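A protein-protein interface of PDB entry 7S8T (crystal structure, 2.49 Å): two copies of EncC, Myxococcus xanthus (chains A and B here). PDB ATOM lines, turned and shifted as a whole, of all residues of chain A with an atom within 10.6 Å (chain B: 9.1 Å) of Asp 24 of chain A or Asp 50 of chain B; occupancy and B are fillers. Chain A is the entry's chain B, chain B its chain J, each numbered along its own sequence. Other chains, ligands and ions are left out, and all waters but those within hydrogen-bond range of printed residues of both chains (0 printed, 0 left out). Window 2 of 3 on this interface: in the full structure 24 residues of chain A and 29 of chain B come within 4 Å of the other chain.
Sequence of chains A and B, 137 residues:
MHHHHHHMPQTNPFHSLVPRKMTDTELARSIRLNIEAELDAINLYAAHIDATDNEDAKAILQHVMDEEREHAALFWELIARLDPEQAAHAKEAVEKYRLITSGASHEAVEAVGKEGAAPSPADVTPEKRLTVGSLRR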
ATOM      1  N   LYS A  21     -35.600  19.811  11.623  1.00  0.00           N
ATOM      2  CA  LYS A  21     -35.138  19.292  12.900  1.00  0.00           C
ATOM      3  C   LYS A  21     -35.501  20.237  14.047  1.00  0.00           C
ATOM      4  O   LYS A  21     -36.621  20.732  14.110  1.00  0.00           O
ATOM      5  CB  LYS A  21     -33.632  19.047  12.843  1.00  0.00           C
ATOM      6  CG  LYS A  21     -33.271  17.978  11.824  1.00  0.00           C
ATOM      7  CD  LYS A  21     -31.779  17.857  11.596  1.00  0.00           C
ATOM      8  CE  LYS A  21     -31.508  17.125  10.287  1.00  0.00           C
ATOM      9  NZ  LYS A  21     -30.060  16.895  10.039  1.00  0.00           N
ATOM     10  N   MET A  22     -34.551  20.466  14.963  1.00  0.00           N
ATOM     11  CA  MET A  22     -34.817  21.376  16.082  1.00  0.00           C
ATOM     12  C   MET A  22     -33.534  21.857  16.758  1.00  0.00           C
ATOM     13  O   MET A  22     -33.606  22.347  17.884  1.00  0.00           O
ATOM     14  CB  MET A  22     -35.730  20.710  17.113  1.00  0.00           C
ATOM     15  N   THR A  23     -32.373  21.694  16.121  1.00  0.00           N
ATOM     16  CA  THR A  23     -31.116  22.274  16.582  1.00  0.00           C
ATOM     17  C   THR A  23     -30.351  22.873  15.404  1.00  0.00           C
ATOM     18  O   THR A  23     -30.000  24.059  15.430  1.00  0.00           O
ATOM     19  CB  THR A  23     -30.262  21.239  17.324  1.00  0.00           C
ATOM     20  OG1 THR A  23     -30.045  20.086  16.495  1.00  0.00           O
ATOM     21  CG2 THR A  23     -30.899  20.832  18.651  1.00  0.00           C
ATOM     22  N   ASP A  24     -30.065  22.074  14.370  1.00  0.00           N
ATOM     23  CA  ASP A  24     -29.302  22.596  13.239  1.00  0.00           C
ATOM     24  C   ASP A  24     -30.187  23.010  12.065  1.00  0.00           C
ATOM     25  O   ASP A  24     -30.411  24.203  11.835  1.00  0.00           O
ATOM     26  CB  ASP A  24     -28.272  21.580  12.749  1.00  0.00           C
ATOM     27  CG  ASP A  24     -27.600  22.014  11.451  1.00  0.00           C
ATOM     28  OD1 ASP A  24     -27.094  23.159  11.389  1.00  0.00           O
ATOM     29  OD2 ASP A  24     -27.596  21.221  10.486  1.00  0.00           O
ATOM     30  N   THR A  25     -30.689  22.015  11.329  1.00  0.00           N
ATOM     31  CA  THR A  25     -31.410  22.247  10.079  1.00  0.00           C
ATOM     32  C   THR A  25     -32.559  23.239  10.235  1.00  0.00           C
ATOM     33  O   THR A  25     -32.569  24.302   9.604  1.00  0.00           O
ATOM     34  CB  THR A  25     -31.930  20.912   9.533  1.00  0.00           C
ATOM     35  OG1 THR A  25     -30.835  20.152   9.004  1.00  0.00           O
ATOM     36  CG2 THR A  25     -32.953  21.138   8.428  1.00  0.00           C
ATOM     37  N   GLU A  26     -33.537  22.910  11.072  1.00  0.00           N
ATOM     38  CA  GLU A  26     -34.691  23.777  11.263  1.00  0.00           C
ATOM     39  C   GLU A  26     -34.510  24.856  12.322  1.00  0.00           C
ATOM     40  O   GLU A  26     -35.426  25.665  12.500  1.00  0.00           O
ATOM     41  CB  GLU A  26     -35.927  22.937  11.607  1.00  0.00           C
ATOM     42  N   LEU A  27     -33.417  24.872  13.079  1.00  0.00           N
ATOM     43  CA  LEU A  27     -33.344  25.925  14.086  1.00  0.00           C
ATOM     44  C   LEU A  27     -32.420  27.089  13.745  1.00  0.00           C
ATOM     45  O   LEU A  27     -32.829  28.241  13.889  1.00  0.00           O
ATOM     46  CB  LEU A  27     -32.958  25.336  15.447  1.00  0.00           C
ATOM     47  CG  LEU A  27     -33.530  26.211  16.563  1.00  0.00           C
ATOM     48  CD1 LEU A  27     -34.954  26.607  16.207  1.00  0.00           C
ATOM     49  CD2 LEU A  27     -33.511  25.497  17.896  1.00  0.00           C
ATOM     50  N   ALA A  28     -31.190  26.844  13.284  1.00  0.00           N
ATOM     51  CA  ALA A  28     -30.285  27.968  13.037  1.00  0.00           C
ATOM     52  C   ALA A  28     -30.633  28.676  11.732  1.00  0.00           C
ATOM     53  O   ALA A  28     -30.725  29.914  11.678  1.00  0.00           O
ATOM     54  CB  ALA A  28     -28.832  27.487  13.018  1.00  0.00           C
ATOM     55  N   ARG A  29     -30.852  27.888  10.677  1.00  0.00           N
ATOM     56  CA  ARG A  29     -31.240  28.444   9.388  1.00  0.00           C
ATOM     57  C   ARG A  29     -32.557  29.199   9.493  1.00  0.00           C
ATOM     58  O   ARG A  29     -32.717  30.281   8.912  1.00  0.00           O
ATOM     59  CB  ARG A  29     -31.384  27.315   8.364  1.00  0.00           C
ATOM     60  CG  ARG A  29     -30.112  26.822   7.712  1.00  0.00           C
ATOM     61  CD  ARG A  29     -30.405  25.557   6.906  1.00  0.00           C
ATOM     62  NE  ARG A  29     -30.801  25.860   5.533  1.00  0.00           N
ATOM     63  CZ  ARG A  29     -32.058  26.040   5.136  1.00  0.00           C
ATOM     64  NH1 ARG A  29     -33.055  25.945   6.006  1.00  0.00           N
ATOM     65  NH2 ARG A  29     -32.322  26.314   3.865  1.00  0.00           N
ATOM     66  N   SER A  30     -33.497  28.656  10.265  1.00  0.00           N
ATOM     67  CA  SER A  30     -34.802  29.284  10.419  1.00  0.00           C
ATOM     68  C   SER A  30     -34.712  30.623  11.137  1.00  0.00           C
ATOM     69  O   SER A  30     -35.416  31.573  10.778  1.00  0.00           O
ATOM     70  CB  SER A  30     -35.735  28.341  11.170  1.00  0.00           C
ATOM     71  OG  SER A  30     -35.381  28.269  12.540  1.00  0.00           O
ATOM     72  N   ILE A  31     -33.848  30.733  12.144  1.00  0.00           N
ATOM     73  CA  ILE A  31     -33.756  31.994  12.866  1.00  0.00           C
ATOM     74  C   ILE A  31     -33.034  33.039  12.024  1.00  0.00           C
ATOM     75  O   ILE A  31     -33.401  34.221  12.031  1.00  0.00           O
ATOM     76  CB  ILE A  31     -33.084  31.782  14.235  1.00  0.00           C
ATOM     77  CG1 ILE A  31     -33.950  30.878  15.117  1.00  0.00           C
ATOM     78  CG2 ILE A  31     -32.833  33.113  14.927  1.00  0.00           C
ATOM     79  CD1 ILE A  31     -35.379  31.352  15.280  1.00  0.00           C
ATOM     80  N   ARG A  32     -32.023  32.627  11.253  1.00  0.00           N
ATOM     81  CA  ARG A  32     -31.435  33.561  10.292  1.00  0.00           C
ATOM     82  C   ARG A  32     -32.481  34.051   9.288  1.00  0.00           C
ATOM     83  O   ARG A  32     -32.514  35.239   8.936  1.00  0.00           O
ATOM     84  CB  ARG A  32     -30.252  32.903   9.583  1.00  0.00           C
ATOM     85  CG  ARG A  32     -29.112  32.519  10.523  1.00  0.00           C
ATOM     86  CD  ARG A  32     -27.880  32.075   9.753  1.00  0.00           C
ATOM     87  NE  ARG A  32     -27.101  31.084  10.488  1.00  0.00           N
ATOM     88  CZ  ARG A  32     -26.654  29.951   9.955  1.00  0.00           C
ATOM     89  NH1 ARG A  32     -26.934  29.662   8.693  1.00  0.00           N
ATOM     90  NH2 ARG A  32     -25.947  29.097  10.683  1.00  0.00           N
ATOM     91  N   LEU A  33     -33.355  33.151   8.823  1.00  0.00           N
ATOM     92  CA  LEU A  33     -34.424  33.557   7.912  1.00  0.00           C
ATOM     93  C   LEU A  33     -35.387  34.537   8.575  1.00  0.00           C
ATOM     94  O   LEU A  33     -35.865  35.482   7.937  1.00  0.00           O
ATOM     95  CB  LEU A  33     -35.185  32.330   7.409  1.00  0.00           C
ATOM     96  CG  LEU A  33     -36.332  32.647   6.445  1.00  0.00           C
ATOM     97  CD1 LEU A  33     -35.786  32.955   5.064  1.00  0.00           C
ATOM     98  CD2 LEU A  33     -37.346  31.513   6.383  1.00  0.00           C
ATOM     99  N   ILE A  79     -29.408  34.059  17.940  1.00  0.00           N
ATOM    100  CA  ILE A  79     -28.597  33.239  17.045  1.00  0.00           C
ATOM    101  C   ILE A  79     -27.150  33.246  17.514  1.00  0.00           C
ATOM    102  O   ILE A  79     -26.412  32.280  17.293  1.00  0.00           O
ATOM    103  CB  ILE A  79     -28.739  33.691  15.574  1.00  0.00           C
ATOM    104  CG1 ILE A  79     -28.067  32.678  14.646  1.00  0.00           C
ATOM    105  CG2 ILE A  79     -28.151  35.068  15.356  1.00  0.00           C
ATOM    106  CD1 ILE A  79     -28.752  31.329  14.623  1.00  0.00           C
ATOM    107  N   LEU A  82     -26.790  30.685  20.417  1.00  0.00           N
ATOM    108  CA  LEU A  82     -27.183  29.371  19.929  1.00  0.00           C
ATOM    109  C   LEU A  82     -25.906  28.600  19.577  1.00  0.00           C
ATOM    110  O   LEU A  82     -24.831  28.889  20.101  1.00  0.00           O
ATOM    111  CB  LEU A  82     -28.162  29.512  18.750  1.00  0.00           C
ATOM    112  CG  LEU A  82     -29.080  28.343  18.399  1.00  0.00           C
ATOM    113  CD1 LEU A  82     -30.214  28.258  19.394  1.00  0.00           C
ATOM    114  CD2 LEU A  82     -29.621  28.474  16.978  1.00  0.00           C
ATOM    115  N   ASP A  83     -26.036  27.605  18.695  1.00  0.00           N
ATOM    116  CA  ASP A  83     -24.859  26.920  18.159  1.00  0.00           C
ATOM    117  C   ASP A  83     -23.863  27.844  17.463  1.00  0.00           C
ATOM    118  O   ASP A  83     -22.649  27.645  17.660  1.00  0.00           O
ATOM    119  CB  ASP A  83     -25.293  25.814  17.182  1.00  0.00           C
ATOM    120  CG  ASP A  83     -26.122  24.727  17.839  1.00  0.00           C
ATOM    121  OD1 ASP A  83     -25.994  24.520  19.062  1.00  0.00           O
ATOM    122  OD2 ASP A  83     -26.912  24.079  17.119  1.00  0.00           O
ATOM    123  N   PRO A  84     -24.264  28.815  16.635  1.00  0.00           N
ATOM    124  CA  PRO A  84     -23.287  29.619  15.885  1.00  0.00           C
ATOM    125  C   PRO A  84     -22.294  30.345  16.780  1.00  0.00           C
ATOM    126  O   PRO A  84     -22.435  30.427  18.002  1.00  0.00           O
ATOM    127  CB  PRO A  84     -24.162  30.612  15.113  1.00  0.00           C
ATOM    128  CG  PRO A  84     -25.447  29.924  14.966  1.00  0.00           C
ATOM    129  CD  PRO A  84     -25.641  29.158  16.231  1.00  0.00           C
ATOM    130  N   ILE B  42     -25.379  31.832   4.416  1.00  0.00           N
ATOM    131  CA  ILE B  42     -24.953  31.025   5.557  1.00  0.00           C
ATOM    132  C   ILE B  42     -25.953  29.901   5.794  1.00  0.00           C
ATOM    133  O   ILE B  42     -25.578  28.786   6.168  1.00  0.00           O
ATOM    134  CB  ILE B  42     -24.756  31.891   6.816  1.00  0.00           C
ATOM    135  CG1 ILE B  42     -23.840  33.077   6.527  1.00  0.00           C
ATOM    136  CG2 ILE B  42     -24.126  31.070   7.928  1.00  0.00           C
ATOM    137  CD1 ILE B  42     -24.055  34.243   7.471  1.00  0.00           C
ATOM    138  N   ASN B  43     -27.243  30.184   5.594  1.00  0.00           N
ATOM    139  CA  ASN B  43     -28.260  29.148   5.743  1.00  0.00           C
ATOM    140  C   ASN B  43     -28.031  28.009   4.755  1.00  0.00           C
ATOM    141  O   ASN B  43     -28.151  26.831   5.113  1.00  0.00           O
ATOM    142  CB  ASN B  43     -29.655  29.741   5.531  1.00  0.00           C
ATOM    143  CG  ASN B  43     -30.235  30.332   6.791  1.00  0.00           C
ATOM    144  OD1 ASN B  43     -29.544  30.459   7.796  1.00  0.00           O
ATOM    145  ND2 ASN B  43     -31.514  30.685   6.749  1.00  0.00           N
ATOM    146  N   LEU B  44     -27.689  28.340   3.510  1.00  0.00           N
ATOM    147  CA  LEU B  44     -27.451  27.287   2.524  1.00  0.00           C
ATOM    148  C   LEU B  44     -26.235  26.453   2.903  1.00  0.00           C
ATOM    149  O   LEU B  44     -26.262  25.221   2.812  1.00  0.00           O
ATOM    150  CB  LEU B  44     -27.284  27.884   1.121  1.00  0.00           C
ATOM    151  CG  LEU B  44     -27.080  26.977  -0.110  1.00  0.00           C
ATOM    152  CD1 LEU B  44     -27.408  27.758  -1.371  1.00  0.00           C
ATOM    153  CD2 LEU B  44     -25.671  26.391  -0.236  1.00  0.00           C
ATOM    154  N   TYR B  45     -25.157  27.106   3.335  1.00  0.00           N
ATOM    155  CA  TYR B  45     -23.962  26.349   3.704  1.00  0.00           C
ATOM    156  C   TYR B  45     -24.210  25.495   4.950  1.00  0.00           C
ATOM    157  O   TYR B  45     -23.644  24.399   5.083  1.00  0.00           O
ATOM    158  CB  TYR B  45     -22.783  27.310   3.877  1.00  0.00           C
ATOM    159  CG  TYR B  45     -22.462  28.074   2.600  1.00  0.00           C
ATOM    160  CD1 TYR B  45     -22.643  27.484   1.353  1.00  0.00           C
ATOM    161  CD2 TYR B  45     -21.996  29.385   2.639  1.00  0.00           C
ATOM    162  CE1 TYR B  45     -22.360  28.169   0.187  1.00  0.00           C
ATOM    163  CE2 TYR B  45     -21.709  30.080   1.471  1.00  0.00           C
ATOM    164  CZ  TYR B  45     -21.895  29.465   0.250  1.00  0.00           C
ATOM    165  OH  TYR B  45     -21.614  30.145  -0.915  1.00  0.00           O
ATOM    166  N   ALA B  46     -25.064  25.971   5.861  1.00  0.00           N
ATOM    167  CA  ALA B  46     -25.457  25.180   7.024  1.00  0.00           C
ATOM    168  C   ALA B  46     -26.300  23.977   6.623  1.00  0.00           C
ATOM    169  O   ALA B  46     -26.258  22.935   7.286  1.00  0.00           O
ATOM    170  CB  ALA B  46     -26.221  26.053   8.018  1.00  0.00           C
ATOM    171  N   ALA B  47     -27.132  24.124   5.593  1.00  0.00           N
ATOM    172  CA  ALA B  47     -27.843  22.957   5.080  1.00  0.00           C
ATOM    173  C   ALA B  47     -26.891  21.976   4.403  1.00  0.00           C
ATOM    174  O   ALA B  47     -27.092  20.758   4.480  1.00  0.00           O
ATOM    175  CB  ALA B  47     -28.938  23.392   4.106  1.00  0.00           C
ATOM    176  N   HIS B  48     -25.842  22.488   3.760  1.00  0.00           N
ATOM    177  CA  HIS B  48     -24.893  21.653   3.028  1.00  0.00           C
ATOM    178  C   HIS B  48     -23.827  20.977   3.891  1.00  0.00           C
ATOM    179  O   HIS B  48     -23.196  20.028   3.416  1.00  0.00           O
ATOM    180  CB  HIS B  48     -24.239  22.471   1.920  1.00  0.00           C
ATOM    181  CG  HIS B  48     -25.059  22.515   0.670  1.00  0.00           C
ATOM    182  ND1 HIS B  48     -26.395  22.854   0.674  1.00  0.00           N
ATOM    183  CD2 HIS B  48     -24.743  22.235  -0.615  1.00  0.00           C
ATOM    184  CE1 HIS B  48     -26.865  22.797  -0.559  1.00  0.00           C
ATOM    185  NE2 HIS B  48     -25.883  22.424  -1.359  1.00  0.00           N
ATOM    186  N   ILE B  49     -23.605  21.417   5.133  1.00  0.00           N
ATOM    187  CA  ILE B  49     -22.613  20.726   5.966  1.00  0.00           C
ATOM    188  C   ILE B  49     -23.028  19.282   6.229  1.00  0.00           C
ATOM    189  O   ILE B  49     -22.190  18.374   6.235  1.00  0.00           O
ATOM    190  CB  ILE B  49     -22.382  21.484   7.295  1.00  0.00           C
ATOM    191  CG1 ILE B  49     -21.281  20.809   8.128  1.00  0.00           C
ATOM    192  CG2 ILE B  49     -23.658  21.603   8.104  1.00  0.00           C
ATOM    193  CD1 ILE B  49     -20.843  21.601   9.358  1.00  0.00           C
ATOM    194  N   ASP B  50     -24.321  19.034   6.413  1.00  0.00           N
ATOM    195  CA  ASP B  50     -24.830  17.704   6.731  1.00  0.00           C
ATOM    196  C   ASP B  50     -25.382  16.969   5.512  1.00  0.00           C
ATOM    197  O   ASP B  50     -26.294  16.147   5.649  1.00  0.00           O
ATOM    198  CB  ASP B  50     -25.872  17.781   7.847  1.00  0.00           C
ATOM    199  CG  ASP B  50     -25.245  18.102   9.197  1.00  0.00           C
ATOM    200  OD1 ASP B  50     -24.379  17.322   9.649  1.00  0.00           O
ATOM    201  OD2 ASP B  50     -25.607  19.135   9.800  1.00  0.00           O
ATOM    202  N   ALA B  51     -24.849  17.243   4.317  1.00  0.00           N
ATOM    203  CA  ALA B  51     -25.379  16.653   3.091  1.00  0.00           C
ATOM    204  C   ALA B  51     -24.345  15.857   2.300  1.00  0.00           C
ATOM    205  O   ALA B  51     -24.551  15.606   1.108  1.00  0.00           O
ATOM    206  CB  ALA B  51     -25.981  17.745   2.204  1.00  0.00           C
ATOM    207  N   THR B  52     -23.243  15.447   2.924  1.00  0.00           N
ATOM    208  CA  THR B  52     -22.253  14.612   2.253  1.00  0.00           C
ATOM    209  C   THR B  52     -21.375  13.948   3.303  1.00  0.00           C
ATOM    210  O   THR B  52     -21.474  14.237   4.498  1.00  0.00           O
ATOM    211  CB  THR B  52     -21.389  15.415   1.273  1.00  0.00           C
ATOM    212  OG1 THR B  52     -20.454  14.536   0.631  1.00  0.00           O
ATOM    213  CG2 THR B  52     -20.623  16.502   2.005  1.00  0.00           C
ATOM    214  N   ASP B  53     -20.504  13.052   2.836  1.00  0.00           N
ATOM    215  CA  ASP B  53     -19.481  12.458   3.685  1.00  0.00           C
ATOM    216  C   ASP B  53     -18.105  12.671   3.069  1.00  0.00           C
ATOM    217  O   ASP B  53     -17.206  11.842   3.215  1.00  0.00           O
ATOM    218  CB  ASP B  53     -19.739  10.971   3.938  1.00  0.00           C
ATOM    219  CG  ASP B  53     -19.753  10.149   2.665  1.00  0.00           C
ATOM    220  OD1 ASP B  53     -19.800  10.741   1.567  1.00  0.00           O
ATOM    221  OD2 ASP B  53     -19.711   8.904   2.762  1.00  0.00           O
ATOM    222  N   ASN B  54     -17.942  13.793   2.377  1.00  0.00           N
ATOM    223  CA  ASN B  54     -16.634  14.233   1.935  1.00  0.00           C
ATOM    224  C   ASN B  54     -16.123  15.109   3.065  1.00  0.00           C
ATOM    225  O   ASN B  54     -16.899  15.840   3.683  1.00  0.00           O
ATOM    226  CB  ASN B  54     -16.721  15.028   0.629  1.00  0.00           C
ATOM    227  CG  ASN B  54     -16.684  14.143  -0.607  1.00  0.00           C
ATOM    228  OD1 ASN B  54     -15.878  13.218  -0.701  1.00  0.00           O
ATOM    229  ND2 ASN B  54     -17.559  14.431  -1.566  1.00  0.00           N
ATOM    230  N   LYS B  58     -16.466  19.439   2.974  1.00  0.00           N
ATOM    231  CA  LYS B  58     -17.135  19.915   4.183  1.00  0.00           C
ATOM    232  C   LYS B  58     -16.292  20.969   4.890  1.00  0.00           C
ATOM    233  O   LYS B  58     -16.823  21.960   5.401  1.00  0.00           O
ATOM    234  CB  LYS B  58     -17.446  18.743   5.117  1.00  0.00           C
ATOM    235  CG  LYS B  58     -18.784  18.073   4.831  1.00  0.00           C
ATOM    236  CD  LYS B  58     -18.996  16.846   5.707  1.00  0.00           C
ATOM    237  CE  LYS B  58     -19.115  17.219   7.172  1.00  0.00           C
ATOM    238  NZ  LYS B  58     -20.481  17.703   7.498  1.00  0.00           N
ATOM    239  N   LEU B  61     -16.387  24.213   3.024  1.00  0.00           N
ATOM    240  CA  LEU B  61     -17.712  24.792   3.210  1.00  0.00           C
ATOM    241  C   LEU B  61     -17.853  25.424   4.586  1.00  0.00           C
ATOM    242  O   LEU B  61     -18.472  26.479   4.719  1.00  0.00           O
ATOM    243  CB  LEU B  61     -18.788  23.733   2.972  1.00  0.00           C
ATOM    244  CG  LEU B  61     -19.362  23.588   1.560  1.00  0.00           C
ATOM    245  CD1 LEU B  61     -20.200  24.817   1.259  1.00  0.00           C
ATOM    246  CD2 LEU B  61     -18.281  23.439   0.498  1.00  0.00           C
ATOM    247  N   MET B  65     -18.483  29.292   5.112  1.00  0.00           N
ATOM    248  CA  MET B  65     -19.635  29.608   5.941  1.00  0.00           C
ATOM    249  C   MET B  65     -19.264  30.534   7.089  1.00  0.00           C
ATOM    250  O   MET B  65     -19.982  31.497   7.375  1.00  0.00           O
ATOM    251  CB  MET B  65     -20.240  28.307   6.464  1.00  0.00           C
ATOM    252  CG  MET B  65     -21.490  28.490   7.257  1.00  0.00           C
ATOM    253  SD  MET B  65     -22.242  26.917   7.670  1.00  0.00           S
ATOM    254  CE  MET B  65     -23.269  27.459   9.024  1.00  0.00           C
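Of the 17 printed residues of chain A, 4 touch a printed residue of chain B. Printed residues of chain A that touch a printed residue of chain B: Asp 24, Arg 29, Arg 32 and Leu 33. Hydrophobic or aromatic side chains of chain B within 4 Å of the printed part of chain A: Ile 42, Ala 46, Ala 47 and Met 65. Among the printed residues, no Asp or Glu carboxylate lies within 4 Å of a Lys or Arg side-chain nitrogen of the other chain.
The backbone NH of Ala 46 of chain B lies within hydrogen-bond range of the side-chain sulfur of Met 65 of chain B (3.5 Å).
Ala 46 of chain B touches Asp 24 of chain A (O to OD2, 3.9 Å). Arg 29 of chain A touches Ala 46 of chain B. Arg 29 of chain A touches Ala 47 of chain B (NE to CB, 3.4 Å). Arg 32 of chain A touches Ala 46 of chain B (NH1 to CB, 3.7 Å). Met 65 of chain B touches Arg 32 of chain A. Asn 43 of chain B touches Leu 33 of chain A.
Asp 24 of chain A touches just these residues of chain B: Ala 46 and Asp 50. Of chain A, only Asp 24 comes within 4 Å of Asp 50 of chain B. Ala 46 of chain B touches just these residues of chain A: Asp 24, Arg 29 and Arg 32. Ile 49 of chain B touches none of the printed residues of chain A. No residue of chain A comes within 4 Å of Ala 51 of chain B. Printed residues of chain A within 4 Å of Met 65 of chain B: Arg 32. Of the printed residues of chain B, Arg 32 of chain A touches Ile 42 (3.0 Å), Asn 43 (2.9 Å), Ala 46 (3.7 Å) and Met 65 (3.6 Å). Of the printed residues of chain A, Ile 42 of chain B touches Arg 32 (3.0 Å). Of the printed residues of chain A, Asn 43 of chain B touches Arg 29, Arg 32 and Leu 33. Tyr 45 of chain B touches none of the printed residues of chain A. The nearest residue of chain A that does not touch Asp 50 of chain B is Lys 21 of chain A (4.8 Å). The nearest printed residue of chain A that does not touch Asn 43 of chain B is Ala 28 of chain A (4.1 Å).
No position is printed for both chains. Of the 10 pairs that touch across the chains among the printed residues, none has its exchanged pair printed and touching as well.
The side-chain carboxylate (OD2) of Asp 24 of chain A lies close to the side-chain carboxylate (OD2) of Asp 50 of chain B, 3.0 Å away. The guanidinium group (NH1) of Arg 32 of chain A lies within hydrogen-bond range of the side-chain amide oxygen (OD1) of Asn 43 of chain B, 2.9 Å away. NH1 of Arg 32 of chain A sits at hydrogen-bond distance from O of Ile 42 of chain B, 3.0 Å away. The backbone carbonyl oxygen of Arg 29 of chain A sits at hydrogen-bond distance from the side-chain amide nitrogen of Asn 43 of chain B (2.5 Å).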
